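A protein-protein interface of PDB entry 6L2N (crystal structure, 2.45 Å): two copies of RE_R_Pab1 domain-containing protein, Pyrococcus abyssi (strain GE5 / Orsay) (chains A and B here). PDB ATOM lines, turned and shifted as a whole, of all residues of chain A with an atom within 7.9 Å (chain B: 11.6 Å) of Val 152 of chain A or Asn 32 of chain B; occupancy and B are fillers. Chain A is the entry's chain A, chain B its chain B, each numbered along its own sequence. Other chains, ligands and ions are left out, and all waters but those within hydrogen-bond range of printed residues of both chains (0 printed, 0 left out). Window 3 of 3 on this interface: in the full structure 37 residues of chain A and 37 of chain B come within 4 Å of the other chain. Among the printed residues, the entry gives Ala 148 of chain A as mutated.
The side-chain amide oxygen (OE1) of Gln 149 of chain A sits close to the side-chain amide oxygen (OE1) of Gln 155 of chain A (3.3 Å).
Val 34 of chain B touches His 147 of chain A (CG1 to NE2, 3.6 Å).
CD of Pro 37 of chain B touches O of Gln 149 of chain A, 3.2 Å away.
CG of Pro 37 of chain B touches NH1 of Arg 150 of chain A, at 3.3 Å.
CG2 of Val 152 of chain A touches CB of Asn 32 of chain B, at 3.5 Å.
Val 152 of chain A touches Val 34 of chain B.
Of the printed residues of chain B, Arg 150 of chain A touches Pro 37.
Ala 151 of chain A touches none of the printed residues of chain B.
Of chain B, only Asn 32 (3.5 Å) and Val 34 (3.7 Å) come within 4 Å of Val 152 of chain A.
No residue of chain B comes within 4 Å of Gly 153 of chain A.
Gln 155 of chain A touches none of the printed residues of chain B.
Asn 32 of chain B touches one residue of chain A.
Printed residues of chain A within 4 Å of Val 34 of chain B: His 147 and Val 152.
Printed residues of chain A within 4 Å of Pro 37 of chain B: Gln 149 and Arg 150.
Hydrophobic or aromatic side chains of chain B that line the printed part of chain A: Val 34 and Pro 37.
Of the 9 printed residues of chain A, 4 touch a printed residue of chain B.
Printed residues of chain A that touch a printed residue of chain B: His 147, Gln 149, Arg 150 and Val 152.
Hydrophobic or aromatic side chains of chain A within 4 Å of the printed part of chain B: His 147 and Val 152.
Among the printed residues, 5 pairs touch across the chains.
No position is printed for both chains.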
ATOM      1  N   HIS A 147       3.409 -16.566  17.349  1.00  0.00           N
ATOM      2  CA  HIS A 147       3.609 -15.715  16.186  1.00  0.00           C
ATOM      3  C   HIS A 147       4.830 -14.828  16.388  1.00  0.00           C
ATOM      4  O   HIS A 147       5.009 -14.235  17.456  1.00  0.00           O
ATOM      5  CB  HIS A 147       2.371 -14.852  15.944  1.00  0.00           C
ATOM      6  CG  HIS A 147       1.332 -15.506  15.087  1.00  0.00           C
ATOM      7  ND1 HIS A 147       0.126 -15.948  15.587  1.00  0.00           N
ATOM      8  CD2 HIS A 147       1.315 -15.782  13.762  1.00  0.00           C
ATOM      9  CE1 HIS A 147      -0.588 -16.472  14.607  1.00  0.00           C
ATOM     10  NE2 HIS A 147       0.111 -16.384  13.489  1.00  0.00           N
ATOM     11  N   ALA A 148       5.678 -14.743  15.365  1.00  0.00           N
ATOM     12  CA  ALA A 148       6.742 -13.746  15.362  1.00  0.00           C
ATOM     13  C   ALA A 148       6.097 -12.371  15.266  1.00  0.00           C
ATOM     14  O   ALA A 148       5.540 -12.014  14.225  1.00  0.00           O
ATOM     15  CB  ALA A 148       7.708 -13.990  14.208  1.00  0.00           C
ATOM     16  N   GLN A 149       6.154 -11.603  16.357  1.00  0.00           N
ATOM     17  CA  GLN A 149       5.355 -10.384  16.446  1.00  0.00           C
ATOM     18  C   GLN A 149       5.779  -9.347  15.413  1.00  0.00           C
ATOM     19  O   GLN A 149       4.928  -8.681  14.814  1.00  0.00           O
ATOM     20  CB  GLN A 149       5.435  -9.805  17.861  1.00  0.00           C
ATOM     21  CG  GLN A 149       6.852  -9.599  18.375  1.00  0.00           C
ATOM     22  CD  GLN A 149       7.344 -10.768  19.204  1.00  0.00           C
ATOM     23  OE1 GLN A 149       7.749 -11.798  18.665  1.00  0.00           O
ATOM     24  NE2 GLN A 149       7.318 -10.613  20.523  1.00  0.00           N
ATOM     25  N   ARG A 150       7.083  -9.195  15.186  1.00  0.00           N
ATOM     26  CA  ARG A 150       7.540  -8.145  14.281  1.00  0.00           C
ATOM     27  C   ARG A 150       7.476  -8.581  12.821  1.00  0.00           C
ATOM     28  O   ARG A 150       7.125  -7.778  11.949  1.00  0.00           O
ATOM     29  CB  ARG A 150       8.958  -7.707  14.651  1.00  0.00           C
ATOM     30  CG  ARG A 150       8.984  -6.648  15.742  1.00  0.00           C
ATOM     31  CD  ARG A 150       7.940  -5.575  15.466  1.00  0.00           C
ATOM     32  NE  ARG A 150       7.856  -4.572  16.525  1.00  0.00           N
ATOM     33  CZ  ARG A 150       7.160  -4.725  17.647  1.00  0.00           C
ATOM     34  NH1 ARG A 150       6.491  -5.849  17.869  1.00  0.00           N
ATOM     35  NH2 ARG A 150       7.136  -3.756  18.551  1.00  0.00           N
ATOM     36  N   ALA A 151       7.803  -9.835  12.534  1.00  0.00           N
ATOM     37  CA  ALA A 151       7.739 -10.366  11.184  1.00  0.00           C
ATOM     38  C   ALA A 151       6.433 -11.148  11.009  1.00  0.00           C
ATOM     39  O   ALA A 151       5.474 -10.956  11.764  1.00  0.00           O
ATOM     40  CB  ALA A 151       8.983 -11.222  10.917  1.00  0.00           C
ATOM     41  N   VAL A 152       6.379 -12.013  10.002  1.00  0.00           N
ATOM     42  CA  VAL A 152       5.325 -13.012   9.903  1.00  0.00           C
ATOM     43  C   VAL A 152       5.987 -14.379   9.824  1.00  0.00           C
ATOM     44  O   VAL A 152       7.096 -14.530   9.302  1.00  0.00           O
ATOM     45  CB  VAL A 152       4.366 -12.772   8.711  1.00  0.00           C
ATOM     46  CG1 VAL A 152       4.907 -13.379   7.425  1.00  0.00           C
ATOM     47  CG2 VAL A 152       2.988 -13.332   9.035  1.00  0.00           C
ATOM     48  N   GLY A 153       5.307 -15.371  10.373  1.00  0.00           N
ATOM     49  CA  GLY A 153       5.885 -16.663  10.669  1.00  0.00           C
ATOM     50  C   GLY A 153       5.837 -16.931  12.157  1.00  0.00           C
ATOM     51  O   GLY A 153       5.212 -16.198  12.930  1.00  0.00           O
ATOM     52  N   TYR A 154       6.520 -17.992  12.568  1.00  0.00           N
ATOM     53  CA  TYR A 154       6.510 -18.408  13.960  1.00  0.00           C
ATOM     54  C   TYR A 154       7.906 -18.327  14.557  1.00  0.00           C
ATOM     55  O   TYR A 154       8.915 -18.413  13.849  1.00  0.00           O
ATOM     56  CB  TYR A 154       5.972 -19.836  14.111  1.00  0.00           C
ATOM     57  CG  TYR A 154       4.705 -20.093  13.332  1.00  0.00           C
ATOM     58  CD1 TYR A 154       3.510 -19.482  13.691  1.00  0.00           C
ATOM     59  CD2 TYR A 154       4.703 -20.941  12.234  1.00  0.00           C
ATOM     60  CE1 TYR A 154       2.348 -19.714  12.979  1.00  0.00           C
ATOM     61  CE2 TYR A 154       3.548 -21.180  11.518  1.00  0.00           C
ATOM     62  CZ  TYR A 154       2.373 -20.564  11.895  1.00  0.00           C
ATOM     63  OH  TYR A 154       1.221 -20.800  11.180  1.00  0.00           O
ATOM     64  N   GLN A 155       7.948 -18.143  15.871  1.00  0.00           N
ATOM     65  CA  GLN A 155       9.150 -18.338  16.661  1.00  0.00           C
ATOM     66  C   GLN A 155       8.818 -19.307  17.784  1.00  0.00           C
ATOM     67  O   GLN A 155       7.768 -19.195  18.423  1.00  0.00           O
ATOM     68  CB  GLN A 155       9.695 -17.014  17.223  1.00  0.00           C
ATOM     69  CG  GLN A 155       8.708 -16.220  18.061  1.00  0.00           C
ATOM     70  CD  GLN A 155       9.373 -15.096  18.836  1.00  0.00           C
ATOM     71  OE1 GLN A 155       8.851 -14.632  19.849  1.00  0.00           O
ATOM     72  NE2 GLN A 155      10.532 -14.654  18.359  1.00  0.00           N
ATOM     73  N   LYS B  28      -1.787  -0.979  13.688  1.00  0.00           N
ATOM     74  CA  LYS B  28      -1.346  -2.239  13.114  1.00  0.00           C
ATOM     75  C   LYS B  28      -1.766  -2.309  11.652  1.00  0.00           C
ATOM     76  O   LYS B  28      -2.640  -1.567  11.196  1.00  0.00           O
ATOM     77  CB  LYS B  28      -1.928  -3.435  13.880  1.00  0.00           C
ATOM     78  CG  LYS B  28      -1.335  -3.610  15.266  1.00  0.00           C
ATOM     79  CD  LYS B  28      -0.952  -5.057  15.492  1.00  0.00           C
ATOM     80  CE  LYS B  28      -1.931  -5.731  16.428  1.00  0.00           C
ATOM     81  NZ  LYS B  28      -1.595  -5.438  17.844  1.00  0.00           N
ATOM     82  N   LYS B  29      -1.125  -3.213  10.915  1.00  0.00           N
ATOM     83  CA  LYS B  29      -1.458  -3.465   9.519  1.00  0.00           C
ATOM     84  C   LYS B  29      -1.642  -4.960   9.326  1.00  0.00           C
ATOM     85  O   LYS B  29      -0.821  -5.756   9.793  1.00  0.00           O
ATOM     86  CB  LYS B  29      -0.368  -2.938   8.581  1.00  0.00           C
ATOM     87  CG  LYS B  29      -0.125  -3.806   7.357  1.00  0.00           C
ATOM     88  CD  LYS B  29       0.943  -3.218   6.451  1.00  0.00           C
ATOM     89  CE  LYS B  29       1.269  -4.166   5.312  1.00  0.00           C
ATOM     90  NZ  LYS B  29       0.043  -4.830   4.794  1.00  0.00           N
ATOM     91  N   ILE B  30      -2.723  -5.338   8.650  1.00  0.00           N
ATOM     92  CA  ILE B  30      -2.952  -6.741   8.334  1.00  0.00           C
ATOM     93  C   ILE B  30      -1.928  -7.179   7.296  1.00  0.00           C
ATOM     94  O   ILE B  30      -1.850  -6.615   6.200  1.00  0.00           O
ATOM     95  CB  ILE B  30      -4.384  -6.969   7.836  1.00  0.00           C
ATOM     96  CG1 ILE B  30      -5.383  -6.801   8.985  1.00  0.00           C
ATOM     97  CG2 ILE B  30      -4.515  -8.351   7.209  1.00  0.00           C
ATOM     98  CD1 ILE B  30      -6.820  -7.056   8.586  1.00  0.00           C
ATOM     99  N   GLU B  31      -1.128  -8.183   7.645  1.00  0.00           N
ATOM    100  CA  GLU B  31      -0.147  -8.756   6.730  1.00  0.00           C
ATOM    101  C   GLU B  31      -0.145 -10.263   6.929  1.00  0.00           C
ATOM    102  O   GLU B  31       0.068 -10.738   8.048  1.00  0.00           O
ATOM    103  CB  GLU B  31       1.251  -8.176   6.965  1.00  0.00           C
ATOM    104  CG  GLU B  31       2.332  -8.823   6.113  1.00  0.00           C
ATOM    105  CD  GLU B  31       3.216  -7.808   5.416  1.00  0.00           C
ATOM    106  OE1 GLU B  31       4.451  -7.870   5.593  1.00  0.00           O
ATOM    107  OE2 GLU B  31       2.678  -6.949   4.688  1.00  0.00           O
ATOM    108  N   ASN B  32      -0.389 -11.004   5.847  1.00  0.00           N
ATOM    109  CA  ASN B  32      -0.522 -12.460   5.897  1.00  0.00           C
ATOM    110  C   ASN B  32      -1.617 -12.888   6.874  1.00  0.00           C
ATOM    111  O   ASN B  32      -1.547 -13.962   7.476  1.00  0.00           O
ATOM    112  CB  ASN B  32       0.811 -13.129   6.248  1.00  0.00           C
ATOM    113  CG  ASN B  32       0.854 -14.596   5.862  1.00  0.00           C
ATOM    114  OD1 ASN B  32       1.629 -15.374   6.416  1.00  0.00           O
ATOM    115  ND2 ASN B  32       0.014 -14.980   4.908  1.00  0.00           N
ATOM    116  N   GLY B  33      -2.633 -12.040   7.047  1.00  0.00           N
ATOM    117  CA  GLY B  33      -3.770 -12.353   7.884  1.00  0.00           C
ATOM    118  C   GLY B  33      -3.631 -11.986   9.347  1.00  0.00           C
ATOM    119  O   GLY B  33      -4.637 -12.002  10.068  1.00  0.00           O
ATOM    120  N   VAL B  34      -2.429 -11.657   9.813  1.00  0.00           N
ATOM    121  CA  VAL B  34      -2.204 -11.327  11.214  1.00  0.00           C
ATOM    122  C   VAL B  34      -1.841  -9.853  11.328  1.00  0.00           C
ATOM    123  O   VAL B  34      -1.214  -9.271  10.435  1.00  0.00           O
ATOM    124  CB  VAL B  34      -1.107 -12.209  11.844  1.00  0.00           C
ATOM    125  CG1 VAL B  34      -1.588 -13.646  11.968  1.00  0.00           C
ATOM    126  CG2 VAL B  34       0.171 -12.138  11.026  1.00  0.00           C
ATOM    127  N   GLY B  35      -2.248  -9.247  12.443  1.00  0.00           N
ATOM    128  CA  GLY B  35      -1.912  -7.856  12.699  1.00  0.00           C
ATOM    129  C   GLY B  35      -0.473  -7.728  13.157  1.00  0.00           C
ATOM    130  O   GLY B  35      -0.049  -8.390  14.109  1.00  0.00           O
ATOM    131  N   ILE B  36       0.289  -6.881  12.469  1.00  0.00           N
ATOM    132  CA  ILE B  36       1.690  -6.651  12.814  1.00  0.00           C
ATOM    133  C   ILE B  36       1.868  -5.179  13.176  1.00  0.00           C
ATOM    134  O   ILE B  36       1.151  -4.319  12.646  1.00  0.00           O
ATOM    135  CB  ILE B  36       2.627  -7.077  11.670  1.00  0.00           C
ATOM    136  CG1 ILE B  36       2.725  -5.987  10.600  1.00  0.00           C
ATOM    137  CG2 ILE B  36       2.158  -8.388  11.052  1.00  0.00           C
ATOM    138  CD1 ILE B  36       3.752  -6.276   9.523  1.00  0.00           C
ATOM    139  N   PRO B  37       2.778  -4.851  14.089  1.00  0.00           N
ATOM    140  CA  PRO B  37       2.993  -3.442  14.439  1.00  0.00           C
ATOM    141  C   PRO B  37       3.575  -2.659  13.274  1.00  0.00           C
ATOM    142  O   PRO B  37       4.360  -3.173  12.474  1.00  0.00           O
ATOM    143  CB  PRO B  37       3.986  -3.514  15.607  1.00  0.00           C
ATOM    144  CG  PRO B  37       3.826  -4.895  16.155  1.00  0.00           C
ATOM    145  CD  PRO B  37       3.536  -5.756  14.966  1.00  0.00           C
ATOM    146  N   VAL B  38       3.182  -1.390  13.192  1.00  0.00           N
ATOM    147  CA  VAL B  38       3.601  -0.497  12.120  1.00  0.00           C
ATOM    148  C   VAL B  38       4.496   0.582  12.711  1.00  0.00           C
ATOM    149  O   VAL B  38       4.150   1.200  13.726  1.00  0.00           O
ATOM    150  CB  VAL B  38       2.392   0.123  11.398  1.00  0.00           C
ATOM    151  CG1 VAL B  38       2.776   1.435  10.725  1.00  0.00           C
ATOM    152  CG2 VAL B  38       1.837  -0.850  10.381  1.00  0.00           C
ATOM    153  N   LYS B  43       8.094   4.419   7.901  1.00  0.00           N
ATOM    154  CA  LYS B  43       7.492   3.901   6.680  1.00  0.00           C
ATOM    155  C   LYS B  43       6.244   4.708   6.361  1.00  0.00           C
ATOM    156  O   LYS B  43       5.393   4.912   7.233  1.00  0.00           O
ATOM    157  CB  LYS B  43       7.146   2.415   6.822  1.00  0.00           C
ATOM    158  CG  LYS B  43       8.300   1.562   7.325  1.00  0.00           C
ATOM    159  CD  LYS B  43       8.420   0.265   6.545  1.00  0.00           C
ATOM    160  CE  LYS B  43       8.438  -0.935   7.478  1.00  0.00           C
ATOM    161  NZ  LYS B  43       8.466  -2.224   6.733  1.00  0.00           N
ATOM    162  N   ASN B  50      -4.453  -0.486   0.135  1.00  0.00           N
ATOM    163  CA  ASN B  50      -3.797  -1.120   1.274  1.00  0.00           C
ATOM    164  C   ASN B  50      -4.065  -0.382   2.577  1.00  0.00           C
ATOM    165  O   ASN B  50      -3.949  -0.981   3.652  1.00  0.00           O
ATOM    166  CB  ASN B  50      -2.287  -1.216   1.038  1.00  0.00           C
ATOM    167  CG  ASN B  50      -1.929  -2.187  -0.073  1.00  0.00           C
ATOM    168  OD1 ASN B  50      -1.396  -3.268   0.181  1.00  0.00           O
ATOM    169  ND2 ASN B  50      -2.213  -1.804  -1.311  1.00  0.00           N
ATOM    170  N   ASP B  53      -6.036  -2.089   5.105  1.00  0.00           N
ATOM    171  CA  ASP B  53      -5.393  -3.108   5.927  1.00  0.00           C
ATOM    172  C   ASP B  53      -4.790  -2.538   7.202  1.00  0.00           C
ATOM    173  O   ASP B  53      -4.414  -3.312   8.089  1.00  0.00           O
ATOM    174  CB  ASP B  53      -4.309  -3.830   5.125  1.00  0.00           C
ATOM    175  CG  ASP B  53      -4.882  -4.831   4.142  1.00  0.00           C
ATOM    176  OD1 ASP B  53      -6.085  -5.150   4.247  1.00  0.00           O
ATOM    177  OD2 ASP B  53      -4.127  -5.299   3.263  1.00  0.00           O
ATOM    178  N   TYR B  54      -4.686  -1.216   7.313  1.00  0.00           N
ATOM    179  CA  TYR B  54      -4.159  -0.576   8.508  1.00  0.00           C
ATOM    180  C   TYR B  54      -5.291  -0.260   9.473  1.00  0.00           C
ATOM    181  O   TYR B  54      -6.379   0.153   9.060  1.00  0.00           O
ATOM    182  CB  TYR B  54      -3.408   0.709   8.150  1.00  0.00           C
ATOM    183  CG  TYR B  54      -2.085   0.485   7.455  1.00  0.00           C
ATOM    184  CD1 TYR B  54      -2.031  -0.089   6.192  1.00  0.00           C
ATOM    185  CD2 TYR B  54      -0.890   0.852   8.060  1.00  0.00           C
ATOM    186  CE1 TYR B  54      -0.828  -0.297   5.556  1.00  0.00           C
ATOM    187  CE2 TYR B  54       0.321   0.650   7.427  1.00  0.00           C
ATOM    188  CZ  TYR B  54       0.344   0.079   6.173  1.00  0.00           C
ATOM    189  OH  TYR B  54       1.545  -0.127   5.534  1.00  0.00           O
ATOM    190  N   TYR B  55      -5.029  -0.452  10.764  1.00  0.00           N
ATOM    191  CA  TYR B  55      -6.034  -0.177  11.777  1.00  0.00           C
ATOM    192  C   TYR B  55      -5.354   0.169  13.093  1.00  0.00           C
ATOM    193  O   TYR B  55      -4.212  -0.220  13.350  1.00  0.00           O
ATOM    194  CB  TYR B  55      -6.988  -1.364  11.966  1.00  0.00           C
ATOM    195  CG  TYR B  55      -6.342  -2.617  12.522  1.00  0.00           C
ATOM    196  CD1 TYR B  55      -5.628  -3.477  11.697  1.00  0.00           C
ATOM    197  CD2 TYR B  55      -6.460  -2.946  13.866  1.00  0.00           C
ATOM    198  CE1 TYR B  55      -5.043  -4.626  12.198  1.00  0.00           C
ATOM    199  CE2 TYR B  55      -5.879  -4.094  14.376  1.00  0.00           C
ATOM    200  CZ  TYR B  55      -5.171  -4.930  13.536  1.00  0.00           C
ATOM    201  OH  TYR B  55      -4.589  -6.073  14.036  1.00  0.00           O
ATOM    202  N   LYS B 132     -15.613 -12.167  18.778  1.00  0.00           N
ATOM    203  CA  LYS B 132     -15.329 -11.183  17.744  1.00  0.00           C
ATOM    204  C   LYS B 132     -16.631 -10.720  17.109  1.00  0.00           C
ATOM    205  O   LYS B 132     -17.528 -11.529  16.854  1.00  0.00           O
ATOM    206  CB  LYS B 132     -14.398 -11.767  16.674  1.00  0.00           C
ATOM    207  CG  LYS B 132     -13.856 -10.750  15.682  1.00  0.00           C
ATOM    208  CD  LYS B 132     -12.755 -11.358  14.830  1.00  0.00           C
ATOM    209  CE  LYS B 132     -12.164 -10.344  13.867  1.00  0.00           C
ATOM    210  NZ  LYS B 132     -11.045 -10.927  13.074  1.00  0.00           N
